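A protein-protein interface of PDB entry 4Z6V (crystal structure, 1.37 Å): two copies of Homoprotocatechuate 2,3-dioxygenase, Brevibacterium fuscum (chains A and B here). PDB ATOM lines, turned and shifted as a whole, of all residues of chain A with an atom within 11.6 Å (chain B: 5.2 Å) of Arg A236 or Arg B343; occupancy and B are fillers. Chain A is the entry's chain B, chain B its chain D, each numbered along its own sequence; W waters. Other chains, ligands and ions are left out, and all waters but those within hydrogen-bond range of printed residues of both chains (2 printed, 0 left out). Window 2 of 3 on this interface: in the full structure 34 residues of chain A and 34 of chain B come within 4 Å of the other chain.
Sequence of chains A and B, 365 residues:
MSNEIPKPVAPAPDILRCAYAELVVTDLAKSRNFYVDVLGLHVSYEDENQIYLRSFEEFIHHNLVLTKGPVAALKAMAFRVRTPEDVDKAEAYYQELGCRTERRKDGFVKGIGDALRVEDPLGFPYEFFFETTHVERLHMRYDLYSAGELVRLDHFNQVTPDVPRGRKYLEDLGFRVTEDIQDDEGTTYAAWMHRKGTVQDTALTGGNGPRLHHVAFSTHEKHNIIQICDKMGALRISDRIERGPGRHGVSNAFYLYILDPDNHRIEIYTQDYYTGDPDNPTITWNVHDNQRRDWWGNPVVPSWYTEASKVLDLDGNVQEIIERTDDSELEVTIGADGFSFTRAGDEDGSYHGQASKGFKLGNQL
OG1 of Thr B342 sits at hydrogen-bond distance from O of Gly B349, 2.7 Å away. The guanidinium group (NH2) of Arg B343 sits at hydrogen-bond distance from the backbone carbonyl oxygen (O) of Asp B348 (2.9 Å). The side-chain carboxylate (OD2) of Asp B346 lies within salt-bridge range of the guanidinium group (NE) of Arg B343 (2.8 Å). The side-chain carboxylate (OD1) of Asp B289 sits at hydrogen-bond distance from the backbone NH (N) of Gln B291.
No position is printed for both chains.
Among the printed residues, merely in contact across the chains: Gly A233 with Trp B295 (3.4 Å), Ala A234 with Trp B295 (3.4 Å), Arg A236 with Trp B285 (3.9 Å), Ser A238 with Trp B295 (3.9 Å), Ser A238 with Thr B342 (3.6 Å), Asp A239 with Thr B342 (3.6 Å) and Asp A239 with Gly B349 (3.4 Å).
The backbone carbonyl oxygen of Arg A236 lies within hydrogen-bond range of the guanidinium group of Arg B343 (2.8 Å). NH1 of Arg A236 lies within salt-bridge range of OD1 of Asp B289. The backbone carbonyl oxygen of Asp A230 sits at hydrogen-bond distance from the indole nitrogen of Trp B295 (3.1 Å). NE of Arg A236 lies close to NE2 of Gln B291, at 3.4 Å. NH1 of Arg B343 lies within salt-bridge range of OD1 of Asp A239. The backbone carbonyl oxygen (O) of Thr B342 sits at hydrogen-bond distance from the guanidinium group (NH1) of Arg A236 (2.9 Å). The side-chain hydroxyl of Ser A238 sits at hydrogen-bond distance from the side-chain amide oxygen of Gln B291. The side-chain amide nitrogen (NE2) of Gln B291 sits at hydrogen-bond distance from the backbone carbonyl oxygen (O) of Gly A233, at 2.9 Å.
Hydrophobic or aromatic side chains of chain B that line the printed part of chain A: Trp B285 and Trp B295. Among the printed residues, Asp or Glu carboxylates within 4 Å of a Lys or Arg side-chain nitrogen of the other chain: Arg A236 with Asp B289 and Asp A239 with Arg B343.
Of chain B, only Trp B285, Asp B289, Gln B291, Thr B342 and Arg B343 come within 4 Å of Arg A236. Arg B343 touches just these residues of chain A: Arg A236 and Asp A239. Asp B289 touches just one residue of chain A: Arg A236 (2.8 Å). No residue of chain A comes within 4 Å of Phe B341. Ala B344 touches none of the printed residues of chain A. Asp B346 touches none of the printed residues of chain A. No residue of chain A comes within 4 Å of Asp B348. Printed residues of chain A within 4 Å of Trp B295: Asp A230 (3.1 Å), Gly A233 (3.4 Å), Ala A234 (3.4 Å) and Ser A238 (3.9 Å). Printed residues of chain B within 4 Å of Ser A238: Gln B291 (2.6 Å), Trp B295 (3.9 Å) and Thr B342 (3.6 Å). Ile A237 touches none of the printed residues of chain B. The nearest residue of chain B that does not touch Arg A236 is Trp B295 (4.1 Å). The nearest residue of chain A that does not touch Arg B343 is Ile A237 (4.03 Å).
Water W1 bridges OG1 of Thr B342 (2.8 Å) and OG of Ser A238 (2.8 Å). Water W2 bridges the side-chain carboxylate (OD2) of Asp A239 (3.1 Å) and the guanidinium group (NH1) of Arg B343 (3.3 Å).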
ATOM      1  N   LYS A  30      -0.077  -3.255  30.071  1.00  0.00           N
ATOM      2  CA  LYS A  30       0.551  -4.552  29.766  1.00  0.00           C
ATOM      3  C   LYS A  30       1.961  -4.616  30.358  1.00  0.00           C
ATOM      4  O   LYS A  30       2.398  -5.650  30.918  1.00  0.00           O
ATOM      5  CB  LYS A  30       0.560  -4.845  28.272  1.00  0.00           C
ATOM      6  CG  LYS A  30      -0.830  -5.139  27.743  1.00  0.00           C
ATOM      7  CD  LYS A  30      -0.853  -5.740  26.351  1.00  0.00           C
ATOM      8  CE  LYS A  30      -2.294  -5.986  25.897  1.00  0.00           C
ATOM      9  NZ  LYS A  30      -2.391  -6.281  24.434  1.00  0.00           N
ATOM     10  N   ASN A  33       1.728  -5.175  34.089  1.00  0.00           N
ATOM     11  CA  ASN A  33       1.436  -6.567  34.425  1.00  0.00           C
ATOM     12  C   ASN A  33       2.732  -7.403  34.455  1.00  0.00           C
ATOM     13  O   ASN A  33       2.923  -8.231  35.329  1.00  0.00           O
ATOM     14  CB  ASN A  33       0.445  -7.180  33.429  1.00  0.00           C
ATOM     15  CG  ASN A  33       0.075  -8.610  33.777  1.00  0.00           C
ATOM     16  OD1 ASN A  33       0.643  -9.547  33.244  1.00  0.00           O
ATOM     17  ND2 ASN A  33      -0.894  -8.772  34.650  1.00  0.00           N
ATOM     18  N   PHE A  34       3.611  -7.166  33.485  1.00  0.00           N
ATOM     19  CA  PHE A  34       4.868  -7.884  33.397  1.00  0.00           C
ATOM     20  C   PHE A  34       5.760  -7.543  34.591  1.00  0.00           C
ATOM     21  O   PHE A  34       6.249  -8.428  35.284  1.00  0.00           O
ATOM     22  CB  PHE A  34       5.573  -7.577  32.070  1.00  0.00           C
ATOM     23  CG  PHE A  34       6.854  -8.354  31.843  1.00  0.00           C
ATOM     24  CD1 PHE A  34       6.817  -9.673  31.406  1.00  0.00           C
ATOM     25  CD2 PHE A  34       8.091  -7.762  32.041  1.00  0.00           C
ATOM     26  CE1 PHE A  34       7.992 -10.363  31.161  1.00  0.00           C
ATOM     27  CE2 PHE A  34       9.257  -8.460  31.820  1.00  0.00           C
ATOM     28  CZ  PHE A  34       9.204  -9.756  31.383  1.00  0.00           C
ATOM     29  N   VAL A  38       3.973 -10.130  37.190  1.00  0.00           N
ATOM     30  CA  VAL A  38       4.832 -11.274  36.923  1.00  0.00           C
ATOM     31  C   VAL A  38       6.110 -11.189  37.761  1.00  0.00           C
ATOM     32  O   VAL A  38       6.433 -12.127  38.514  1.00  0.00           O
ATOM     33  CB  VAL A  38       5.147 -11.466  35.423  1.00  0.00           C
ATOM     34  CG1 VAL A  38       6.045 -12.689  35.205  1.00  0.00           C
ATOM     35  CG2 VAL A  38       3.854 -11.578  34.651  1.00  0.00           C
ATOM     36  N   GLN A 227      12.430 -20.050  40.139  1.00  0.00           N
ATOM     37  CA  GLN A 227      11.012 -19.716  40.387  1.00  0.00           C
ATOM     38  C   GLN A 227      10.454 -18.793  39.303  1.00  0.00           C
ATOM     39  O   GLN A 227       9.302 -18.949  38.923  1.00  0.00           O
ATOM     40  CB  GLN A 227      10.836 -19.099  41.768  1.00  0.00           C
ATOM     41  CG  GLN A 227       9.518 -18.325  41.936  1.00  0.00           C
ATOM     42  CD  GLN A 227       8.239 -19.168  41.825  1.00  0.00           C
ATOM     43  OE1 GLN A 227       8.255 -20.398  41.869  1.00  0.00           O
ATOM     44  NE2 GLN A 227       7.118 -18.477  41.727  1.00  0.00           N
ATOM     45  N   ILE A 228      11.240 -17.826  38.807  1.00  0.00           N
ATOM     46  CA  ILE A 228      10.719 -16.964  37.740  1.00  0.00           C
ATOM     47  C   ILE A 228      10.367 -17.802  36.515  1.00  0.00           C
ATOM     48  O   ILE A 228       9.299 -17.633  35.925  1.00  0.00           O
ATOM     49  CB  ILE A 228      11.729 -15.860  37.400  1.00  0.00           C
ATOM     50  CG1 ILE A 228      11.885 -14.903  38.603  1.00  0.00           C
ATOM     51  CG2 ILE A 228      11.296 -15.093  36.180  1.00  0.00           C
ATOM     52  CD1 ILE A 228      13.082 -14.002  38.472  1.00  0.00           C
ATOM     53  N   CYS A 229      11.241 -18.748  36.180  1.00  0.00           N
ATOM     54  CA  CYS A 229      10.973 -19.662  35.067  1.00  0.00           C
ATOM     55  C   CYS A 229       9.691 -20.465  35.324  1.00  0.00           C
ATOM     56  O   CYS A 229       8.811 -20.566  34.465  1.00  0.00           O
ATOM     57  CB  CYS A 229      12.150 -20.637  34.868  1.00  0.00           C
ATOM     58  SG  CYS A 229      13.688 -19.857  34.401  1.00  0.00           S
ATOM     59  N   ASP A 230       9.603 -21.036  36.523  1.00  0.00           N
ATOM     60  CA  ASP A 230       8.467 -21.866  36.910  1.00  0.00           C
ATOM     61  C   ASP A 230       7.165 -21.070  36.829  1.00  0.00           C
ATOM     62  O   ASP A 230       6.138 -21.559  36.351  1.00  0.00           O
ATOM     63  CB  ASP A 230       8.661 -22.386  38.313  1.00  0.00           C
ATOM     64  CG  ASP A 230       9.708 -23.488  38.419  1.00  0.00           C
ATOM     65  OD1 ASP A 230      10.002 -24.203  37.423  1.00  0.00           O
ATOM     66  OD2 ASP A 230      10.241 -23.640  39.550  1.00  0.00           O
ATOM     67  N   LYS A 231       7.206 -19.824  37.313  1.00  0.00           N
ATOM     68  CA  LYS A 231       6.031 -18.957  37.292  1.00  0.00           C
ATOM     69  C   LYS A 231       5.613 -18.621  35.861  1.00  0.00           C
ATOM     70  O   LYS A 231       4.430 -18.578  35.541  1.00  0.00           O
ATOM     71  CB  LYS A 231       6.304 -17.686  38.108  1.00  0.00           C
ATOM     72  CG  LYS A 231       5.118 -16.744  38.173  1.00  0.00           C
ATOM     73  CD  LYS A 231       5.380 -15.562  39.097  1.00  0.00           C
ATOM     74  CE  LYS A 231       4.156 -14.689  39.251  1.00  0.00           C
ATOM     75  NZ  LYS A 231       4.375 -13.516  40.131  1.00  0.00           N
ATOM     76  N   MET A 232       6.591 -18.349  35.005  1.00  0.00           N
ATOM     77  CA  MET A 232       6.287 -18.058  33.616  1.00  0.00           C
ATOM     78  C   MET A 232       5.676 -19.261  32.907  1.00  0.00           C
ATOM     79  O   MET A 232       4.756 -19.090  32.108  1.00  0.00           O
ATOM     80  CB  MET A 232       7.538 -17.520  32.901  1.00  0.00           C
ATOM     81  CG  MET A 232       7.923 -16.147  33.430  1.00  0.00           C
ATOM     82  SD  MET A 232       9.382 -15.408  32.692  1.00  0.00           S
ATOM     83  CE  MET A 232       8.749 -15.014  31.051  1.00  0.00           C
ATOM     84  N   GLY A 233       6.108 -20.468  33.265  1.00  0.00           N
ATOM     85  CA  GLY A 233       5.434 -21.659  32.799  1.00  0.00           C
ATOM     86  C   GLY A 233       3.990 -21.751  33.281  1.00  0.00           C
ATOM     87  O   GLY A 233       3.072 -22.005  32.497  1.00  0.00           O
ATOM     88  N   ALA A 234       3.768 -21.458  34.557  1.00  0.00           N
ATOM     89  CA  ALA A 234       2.410 -21.521  35.111  1.00  0.00           C
ATOM     90  C   ALA A 234       1.483 -20.485  34.483  1.00  0.00           C
ATOM     91  O   ALA A 234       0.301 -20.730  34.316  1.00  0.00           O
ATOM     92  CB  ALA A 234       2.458 -21.313  36.598  1.00  0.00           C
ATOM     93  N   LEU A 235       2.039 -19.332  34.138  1.00  0.00           N
ATOM     94  CA  LEU A 235       1.292 -18.284  33.456  1.00  0.00           C
ATOM     95  C   LEU A 235       1.193 -18.518  31.948  1.00  0.00           C
ATOM     96  O   LEU A 235       0.558 -17.718  31.234  1.00  0.00           O
ATOM     97  CB  LEU A 235       1.934 -16.930  33.724  1.00  0.00           C
ATOM     98  CG  LEU A 235       1.879 -16.415  35.178  1.00  0.00           C
ATOM     99  CD1 LEU A 235       2.691 -15.154  35.349  1.00  0.00           C
ATOM    100  CD2 LEU A 235       0.448 -16.150  35.599  1.00  0.00           C
ATOM    101  N   ARG A 236       1.794 -19.601  31.464  1.00  0.00           N
ATOM    102  CA  ARG A 236       1.763 -19.986  30.049  1.00  0.00           C
ATOM    103  C   ARG A 236       2.335 -18.857  29.178  1.00  0.00           C
ATOM    104  O   ARG A 236       1.796 -18.548  28.115  1.00  0.00           O
ATOM    105  CB  ARG A 236       0.362 -20.421  29.617  1.00  0.00           C
ATOM    106  CG  ARG A 236       0.009 -21.810  30.139  1.00  0.00           C
ATOM    107  CD  ARG A 236       0.585 -22.843  29.196  1.00  0.00           C
ATOM    108  NE  ARG A 236       0.479 -24.195  29.703  1.00  0.00           N
ATOM    109  CZ  ARG A 236       0.948 -25.255  29.056  1.00  0.00           C
ATOM    110  NH1 ARG A 236       1.489 -25.129  27.847  1.00  0.00           N
ATOM    111  NH2 ARG A 236       0.863 -26.460  29.610  1.00  0.00           N
ATOM    112  N   ILE A 237       3.437 -18.281  29.672  1.00  0.00           N
ATOM    113  CA  ILE A 237       4.227 -17.281  28.942  1.00  0.00           C
ATOM    114  C   ILE A 237       5.687 -17.710  28.838  1.00  0.00           C
ATOM    115  O   ILE A 237       6.604 -16.873  28.764  1.00  0.00           O
ATOM    116  CB  ILE A 237       4.068 -15.856  29.535  1.00  0.00           C
ATOM    117  CG1 ILE A 237       4.569 -15.761  30.986  1.00  0.00           C
ATOM    118  CG2 ILE A 237       2.643 -15.383  29.389  1.00  0.00           C
ATOM    119  CD1 ILE A 237       4.534 -14.382  31.605  1.00  0.00           C
ATOM    120  N   SER A 238       5.916 -19.035  28.777  1.00  0.00           N
ATOM    121  CA  SER A 238       7.273 -19.538  28.599  1.00  0.00           C
ATOM    122  C   SER A 238       7.925 -19.085  27.287  1.00  0.00           C
ATOM    123  O   SER A 238       9.152 -19.105  27.162  1.00  0.00           O
ATOM    124  CB  SER A 238       7.337 -21.056  28.718  1.00  0.00           C
ATOM    125  OG  SER A 238       6.548 -21.672  27.744  1.00  0.00           O
ATOM    126  N   ASP A 239       7.113 -18.695  26.305  1.00  0.00           N
ATOM    127  CA  ASP A 239       7.637 -18.113  25.060  1.00  0.00           C
ATOM    128  C   ASP A 239       8.350 -16.796  25.283  1.00  0.00           C
ATOM    129  O   ASP A 239       9.074 -16.332  24.397  1.00  0.00           O
ATOM    130  CB  ASP A 239       6.543 -17.984  23.972  1.00  0.00           C
ATOM    131  CG  ASP A 239       5.320 -17.176  24.402  1.00  0.00           C
ATOM    132  OD1 ASP A 239       4.920 -17.205  25.591  1.00  0.00           O
ATOM    133  OD2 ASP A 239       4.700 -16.526  23.501  1.00  0.00           O
ATOM    134  N   ARG A 240       8.167 -16.200  26.461  1.00  0.00           N
ATOM    135  CA  ARG A 240       8.851 -14.957  26.802  1.00  0.00           C
ATOM    136  C   ARG A 240      10.144 -15.204  27.589  1.00  0.00           C
ATOM    137  O   ARG A 240      10.856 -14.230  27.946  1.00  0.00           O
ATOM    138  CB  ARG A 240       7.910 -14.006  27.564  1.00  0.00           C
ATOM    139  CG  ARG A 240       6.553 -13.779  26.884  1.00  0.00           C
ATOM    140  CD  ARG A 240       6.704 -13.345  25.431  1.00  0.00           C
ATOM    141  NE  ARG A 240       7.223 -11.992  25.318  1.00  0.00           N
ATOM    142  CZ  ARG A 240       7.593 -11.423  24.181  1.00  0.00           C
ATOM    143  NH1 ARG A 240       7.571 -12.102  23.046  1.00  0.00           N
ATOM    144  NH2 ARG A 240       7.997 -10.170  24.194  1.00  0.00           N
ATOM    145  N   ILE A 241      10.482 -16.487  27.803  1.00  0.00           N
ATOM    146  CA  ILE A 241      11.801 -16.889  28.256  1.00  0.00           C
ATOM    147  C   ILE A 241      12.671 -17.041  27.024  1.00  0.00           C
ATOM    148  O   ILE A 241      12.410 -17.899  26.188  1.00  0.00           O
ATOM    149  CB  ILE A 241      11.800 -18.201  29.070  1.00  0.00           C
ATOM    150  CG1 ILE A 241      10.956 -18.070  30.350  1.00  0.00           C
ATOM    151  CG2 ILE A 241      13.228 -18.596  29.416  1.00  0.00           C
ATOM    152  CD1 ILE A 241      10.737 -19.381  31.050  1.00  0.00           C
ATOM    153  N   ILE A 258      14.702 -12.866  29.812  1.00  0.00           N
ATOM    154  CA  ILE A 258      13.277 -12.825  29.483  1.00  0.00           C
ATOM    155  C   ILE A 258      12.945 -11.547  28.715  1.00  0.00           C
ATOM    156  O   ILE A 258      13.752 -10.619  28.669  1.00  0.00           O
ATOM    157  CB  ILE A 258      12.416 -12.951  30.768  1.00  0.00           C
ATOM    158  CG1 ILE A 258      12.633 -11.760  31.687  1.00  0.00           C
ATOM    159  CG2 ILE A 258      12.716 -14.275  31.481  1.00  0.00           C
ATOM    160  CD1 ILE A 258      11.841 -11.850  32.974  1.00  0.00           C
ATOM    161  N   LEU A 259      11.785 -11.532  28.062  1.00  0.00           N
ATOM    162  CA  LEU A 259      11.403 -10.449  27.180  1.00  0.00           C
ATOM    163  C   LEU A 259      10.110  -9.805  27.643  1.00  0.00           C
ATOM    164  O   LEU A 259       9.116 -10.511  27.859  1.00  0.00           O
ATOM    165  CB  LEU A 259      11.205 -10.999  25.775  1.00  0.00           C
ATOM    166  CG  LEU A 259      12.422 -11.661  25.128  1.00  0.00           C
ATOM    167  CD1 LEU A 259      11.968 -12.319  23.826  1.00  0.00           C
ATOM    168  CD2 LEU A 259      13.553 -10.668  24.910  1.00  0.00           C
ATOM    169  N   ASP A 260      10.121  -8.482  27.789  1.00  0.00           N
ATOM    170  CA  ASP A 260       8.937  -7.753  28.237  1.00  0.00           C
ATOM    171  C   ASP A 260       7.973  -7.565  27.046  1.00  0.00           C
ATOM    172  O   ASP A 260       8.264  -8.013  25.935  1.00  0.00           O
ATOM    173  CB  ASP A 260       9.338  -6.460  28.983  1.00  0.00           C
ATOM    174  CG  ASP A 260       9.447  -5.218  28.082  1.00  0.00           C
ATOM    175  OD1 ASP A 260       9.402  -5.355  26.832  1.00  0.00           O
ATOM    176  OD2 ASP A 260       9.571  -4.108  28.679  1.00  0.00           O
ATOM    177  N   PRO A 261       6.808  -6.928  27.267  1.00  0.00           N
ATOM    178  CA  PRO A 261       5.794  -6.860  26.206  1.00  0.00           C
ATOM    179  C   PRO A 261       6.210  -6.114  24.921  1.00  0.00           C
ATOM    180  O   PRO A 261       5.643  -6.380  23.841  1.00  0.00           O
ATOM    181  CB  PRO A 261       4.622  -6.182  26.907  1.00  0.00           C
ATOM    182  CG  PRO A 261       4.753  -6.636  28.315  1.00  0.00           C
ATOM    183  CD  PRO A 261       6.237  -6.568  28.573  1.00  0.00           C
ATOM    184  N   ASN A 263       9.413  -6.360  23.909  1.00  0.00           N
ATOM    185  CA  ASN A 263      10.648  -7.086  23.583  1.00  0.00           C
ATOM    186  C   ASN A 263      11.909  -6.510  24.193  1.00  0.00           C
ATOM    187  O   ASN A 263      13.014  -6.918  23.828  1.00  0.00           O
ATOM    188  CB  ASN A 263      10.809  -7.252  22.074  1.00  0.00           C
ATOM    189  CG  ASN A 263       9.603  -7.924  21.457  1.00  0.00           C
ATOM    190  OD1 ASN A 263       8.892  -8.670  22.135  1.00  0.00           O
ATOM    191  ND2 ASN A 263       9.349  -7.651  20.187  1.00  0.00           N
ATOM    192  N   TRP B 285      -0.796 -35.138  28.872  1.00  0.00           N
ATOM    193  CA  TRP B 285      -0.343 -33.976  28.131  1.00  0.00           C
ATOM    194  C   TRP B 285      -0.461 -34.239  26.632  1.00  0.00           C
ATOM    195  O   TRP B 285      -0.259 -35.366  26.165  1.00  0.00           O
ATOM    196  CB  TRP B 285       1.120 -33.714  28.431  1.00  0.00           C
ATOM    197  CG  TRP B 285       1.429 -33.428  29.850  1.00  0.00           C
ATOM    198  CD1 TRP B 285       1.448 -34.329  30.873  1.00  0.00           C
ATOM    199  CD2 TRP B 285       1.804 -32.159  30.421  1.00  0.00           C
ATOM    200  NE1 TRP B 285       1.809 -33.715  32.044  1.00  0.00           N
ATOM    201  CE2 TRP B 285       2.026 -32.379  31.803  1.00  0.00           C
ATOM    202  CE3 TRP B 285       1.930 -30.856  29.912  1.00  0.00           C
ATOM    203  CZ2 TRP B 285       2.400 -31.354  32.680  1.00  0.00           C
ATOM    204  CZ3 TRP B 285       2.313 -29.846  30.784  1.00  0.00           C
ATOM    205  CH2 TRP B 285       2.545 -30.102  32.150  1.00  0.00           C
ATOM    206  N   ASP B 289       2.298 -29.818  23.144  1.00  0.00           N
ATOM    207  CA  ASP B 289       2.437 -28.845  24.235  1.00  0.00           C
ATOM    208  C   ASP B 289       3.916 -28.664  24.565  1.00  0.00           C
ATOM    209  O   ASP B 289       4.555 -29.552  25.122  1.00  0.00           O
ATOM    210  CB  ASP B 289       1.653 -29.329  25.463  1.00  0.00           C
ATOM    211  CG  ASP B 289       1.657 -28.348  26.628  1.00  0.00           C
ATOM    212  OD1 ASP B 289       2.546 -27.472  26.690  1.00  0.00           O
ATOM    213  OD2 ASP B 289       0.734 -28.473  27.463  1.00  0.00           O
ATOM    214  N   GLN B 291       5.370 -27.140  26.810  1.00  0.00           N
ATOM    215  CA  GLN B 291       5.761 -27.164  28.221  1.00  0.00           C
ATOM    216  C   GLN B 291       5.701 -28.567  28.834  1.00  0.00           C
ATOM    217  O   GLN B 291       5.902 -28.695  30.030  1.00  0.00           O
ATOM    218  CB  GLN B 291       4.914 -26.179  29.047  1.00  0.00           C
ATOM    219  CG  GLN B 291       5.068 -24.727  28.590  1.00  0.00           C
ATOM    220  CD  GLN B 291       4.420 -23.664  29.452  1.00  0.00           C
ATOM    221  OE1 GLN B 291       4.468 -22.482  29.096  1.00  0.00           O
ATOM    222  NE2 GLN B 291       3.762 -24.063  30.543  1.00  0.00           N
ATOM    223  N   TRP B 295       9.137 -27.495  31.137  1.00  0.00           N
ATOM    224  CA  TRP B 295       8.062 -26.589  31.524  1.00  0.00           C
ATOM    225  C   TRP B 295       8.335 -25.157  31.068  1.00  0.00           C
ATOM    226  O   TRP B 295       7.404 -24.348  30.885  1.00  0.00           O
ATOM    227  CB  TRP B 295       7.933 -26.654  33.033  1.00  0.00           C
ATOM    228  CG  TRP B 295       6.894 -25.812  33.708  1.00  0.00           C
ATOM    229  CD1 TRP B 295       7.124 -24.872  34.673  1.00  0.00           C
ATOM    230  CD2 TRP B 295       5.480 -25.917  33.580  1.00  0.00           C
ATOM    231  NE1 TRP B 295       5.940 -24.360  35.137  1.00  0.00           N
ATOM    232  CE2 TRP B 295       4.909 -24.976  34.476  1.00  0.00           C
ATOM    233  CE3 TRP B 295       4.620 -26.695  32.778  1.00  0.00           C
ATOM    234  CZ2 TRP B 295       3.517 -24.841  34.629  1.00  0.00           C
ATOM    235  CZ3 TRP B 295       3.255 -26.525  32.920  1.00  0.00           C
ATOM    236  CH2 TRP B 295       2.720 -25.634  33.850  1.00  0.00           C
ATOM    237  N   PHE B 341       3.258 -25.742  20.606  1.00  0.00           N
ATOM    238  CA  PHE B 341       2.631 -24.502  21.057  1.00  0.00           C
ATOM    239  C   PHE B 341       3.002 -24.193  22.509  1.00  0.00           C
ATOM    240  O   PHE B 341       3.351 -25.081  23.297  1.00  0.00           O
ATOM    241  CB  PHE B 341       1.103 -24.591  20.908  1.00  0.00           C
ATOM    242  CG  PHE B 341       0.446 -25.674  21.737  1.00  0.00           C
ATOM    243  CD1 PHE B 341       0.218 -25.483  23.107  1.00  0.00           C
ATOM    244  CD2 PHE B 341       0.015 -26.858  21.143  1.00  0.00           C
ATOM    245  CE1 PHE B 341      -0.401 -26.464  23.862  1.00  0.00           C
ATOM    246  CE2 PHE B 341      -0.624 -27.846  21.909  1.00  0.00           C
ATOM    247  CZ  PHE B 341      -0.814 -27.648  23.263  1.00  0.00           C
ATOM    248  N   THR B 342       2.902 -22.920  22.858  1.00  0.00           N
ATOM    249  CA  THR B 342       2.980 -22.472  24.237  1.00  0.00           C
ATOM    250  C   THR B 342       1.585 -22.449  24.878  1.00  0.00           C
ATOM    251  O   THR B 342       1.384 -22.970  25.978  1.00  0.00           O
ATOM    252  CB  THR B 342       3.640 -21.080  24.310  1.00  0.00           C
ATOM    253  OG1 THR B 342       4.959 -21.161  23.760  1.00  0.00           O
ATOM    254  CG2 THR B 342       3.739 -20.595  25.749  1.00  0.00           C
ATOM    255  N   ARG B 343       0.635 -21.868  24.151  1.00  0.00           N
ATOM    256  CA  ARG B 343      -0.783 -21.835  24.536  1.00  0.00           C
ATOM    257  C   ARG B 343      -1.573 -22.536  23.456  1.00  0.00           C
ATOM    258  O   ARG B 343      -1.463 -22.192  22.252  1.00  0.00           O
ATOM    259  CB  ARG B 343      -1.256 -20.399  24.659  1.00  0.00           C
ATOM    260  CG  ARG B 343      -0.639 -19.662  25.844  1.00  0.00           C
ATOM    261  CD  ARG B 343      -0.768 -18.135  25.694  1.00  0.00           C
ATOM    262  NE  ARG B 343      -0.038 -17.627  24.532  1.00  0.00           N
ATOM    263  CZ  ARG B 343       1.254 -17.332  24.501  1.00  0.00           C
ATOM    264  NH1 ARG B 343       2.015 -17.434  25.580  1.00  0.00           N
ATOM    265  NH2 ARG B 343       1.784 -16.922  23.374  1.00  0.00           N
ATOM    266  N   ALA B 344      -2.377 -23.515  23.863  1.00  0.00           N
ATOM    267  CA  ALA B 344      -3.134 -24.301  22.901  1.00  0.00           C
ATOM    268  C   ALA B 344      -4.008 -23.371  22.049  1.00  0.00           C
ATOM    269  O   ALA B 344      -4.707 -22.490  22.574  1.00  0.00           O
ATOM    270  CB  ALA B 344      -3.999 -25.355  23.605  1.00  0.00           C
ATOM    271  N   GLY B 345      -3.932 -23.547  20.737  1.00  0.00           N
ATOM    272  CA  GLY B 345      -4.683 -22.707  19.812  1.00  0.00           C
ATOM    273  C   GLY B 345      -4.117 -21.336  19.463  1.00  0.00           C
ATOM    274  O   GLY B 345      -4.696 -20.626  18.655  1.00  0.00           O
ATOM    275  N   ASP B 346      -2.992 -20.956  20.054  1.00  0.00           N
ATOM    276  CA  ASP B 346      -2.396 -19.633  19.820  1.00  0.00           C
ATOM    277  C   ASP B 346      -1.195 -19.776  18.894  1.00  0.00           C
ATOM    278  O   ASP B 346      -0.257 -20.512  19.180  1.00  0.00           O
ATOM    279  CB  ASP B 346      -1.971 -19.019  21.153  1.00  0.00           C
ATOM    280  CG  ASP B 346      -1.582 -17.556  21.058  1.00  0.00           C
ATOM    281  OD1 ASP B 346      -1.638 -16.953  19.970  1.00  0.00           O
ATOM    282  OD2 ASP B 346      -1.242 -16.990  22.118  1.00  0.00           O
ATOM    283  N   ASP B 348       0.851 -17.266  18.303  1.00  0.00           N
ATOM    284  CA  ASP B 348       1.947 -16.601  19.022  1.00  0.00           C
ATOM    285  C   ASP B 348       2.570 -17.594  19.991  1.00  0.00           C
ATOM    286  O   ASP B 348       1.875 -18.225  20.793  1.00  0.00           O
ATOM    287  CB  ASP B 348       1.459 -15.384  19.815  1.00  0.00           C
ATOM    288  CG  ASP B 348       1.009 -14.249  18.938  1.00  0.00           C
ATOM    289  OD1 ASP B 348       1.374 -14.205  17.749  1.00  0.00           O
ATOM    290  OD2 ASP B 348       0.285 -13.383  19.455  1.00  0.00           O
ATOM    291  N   GLY B 349       3.886 -17.731  19.938  1.00  0.00           N
ATOM    292  CA  GLY B 349       4.543 -18.690  20.821  1.00  0.00           C
ATOM    293  C   GLY B 349       4.467 -20.119  20.325  1.00  0.00           C
ATOM    294  O   GLY B 349       4.752 -21.064  21.070  1.00  0.00           O
HETATM  295  O   HOH W   1       6.996 -22.431  25.121  1.00  0.00           O
HETATM  296  O   HOH W   2       3.217 -14.405  25.259  1.00  0.00           O
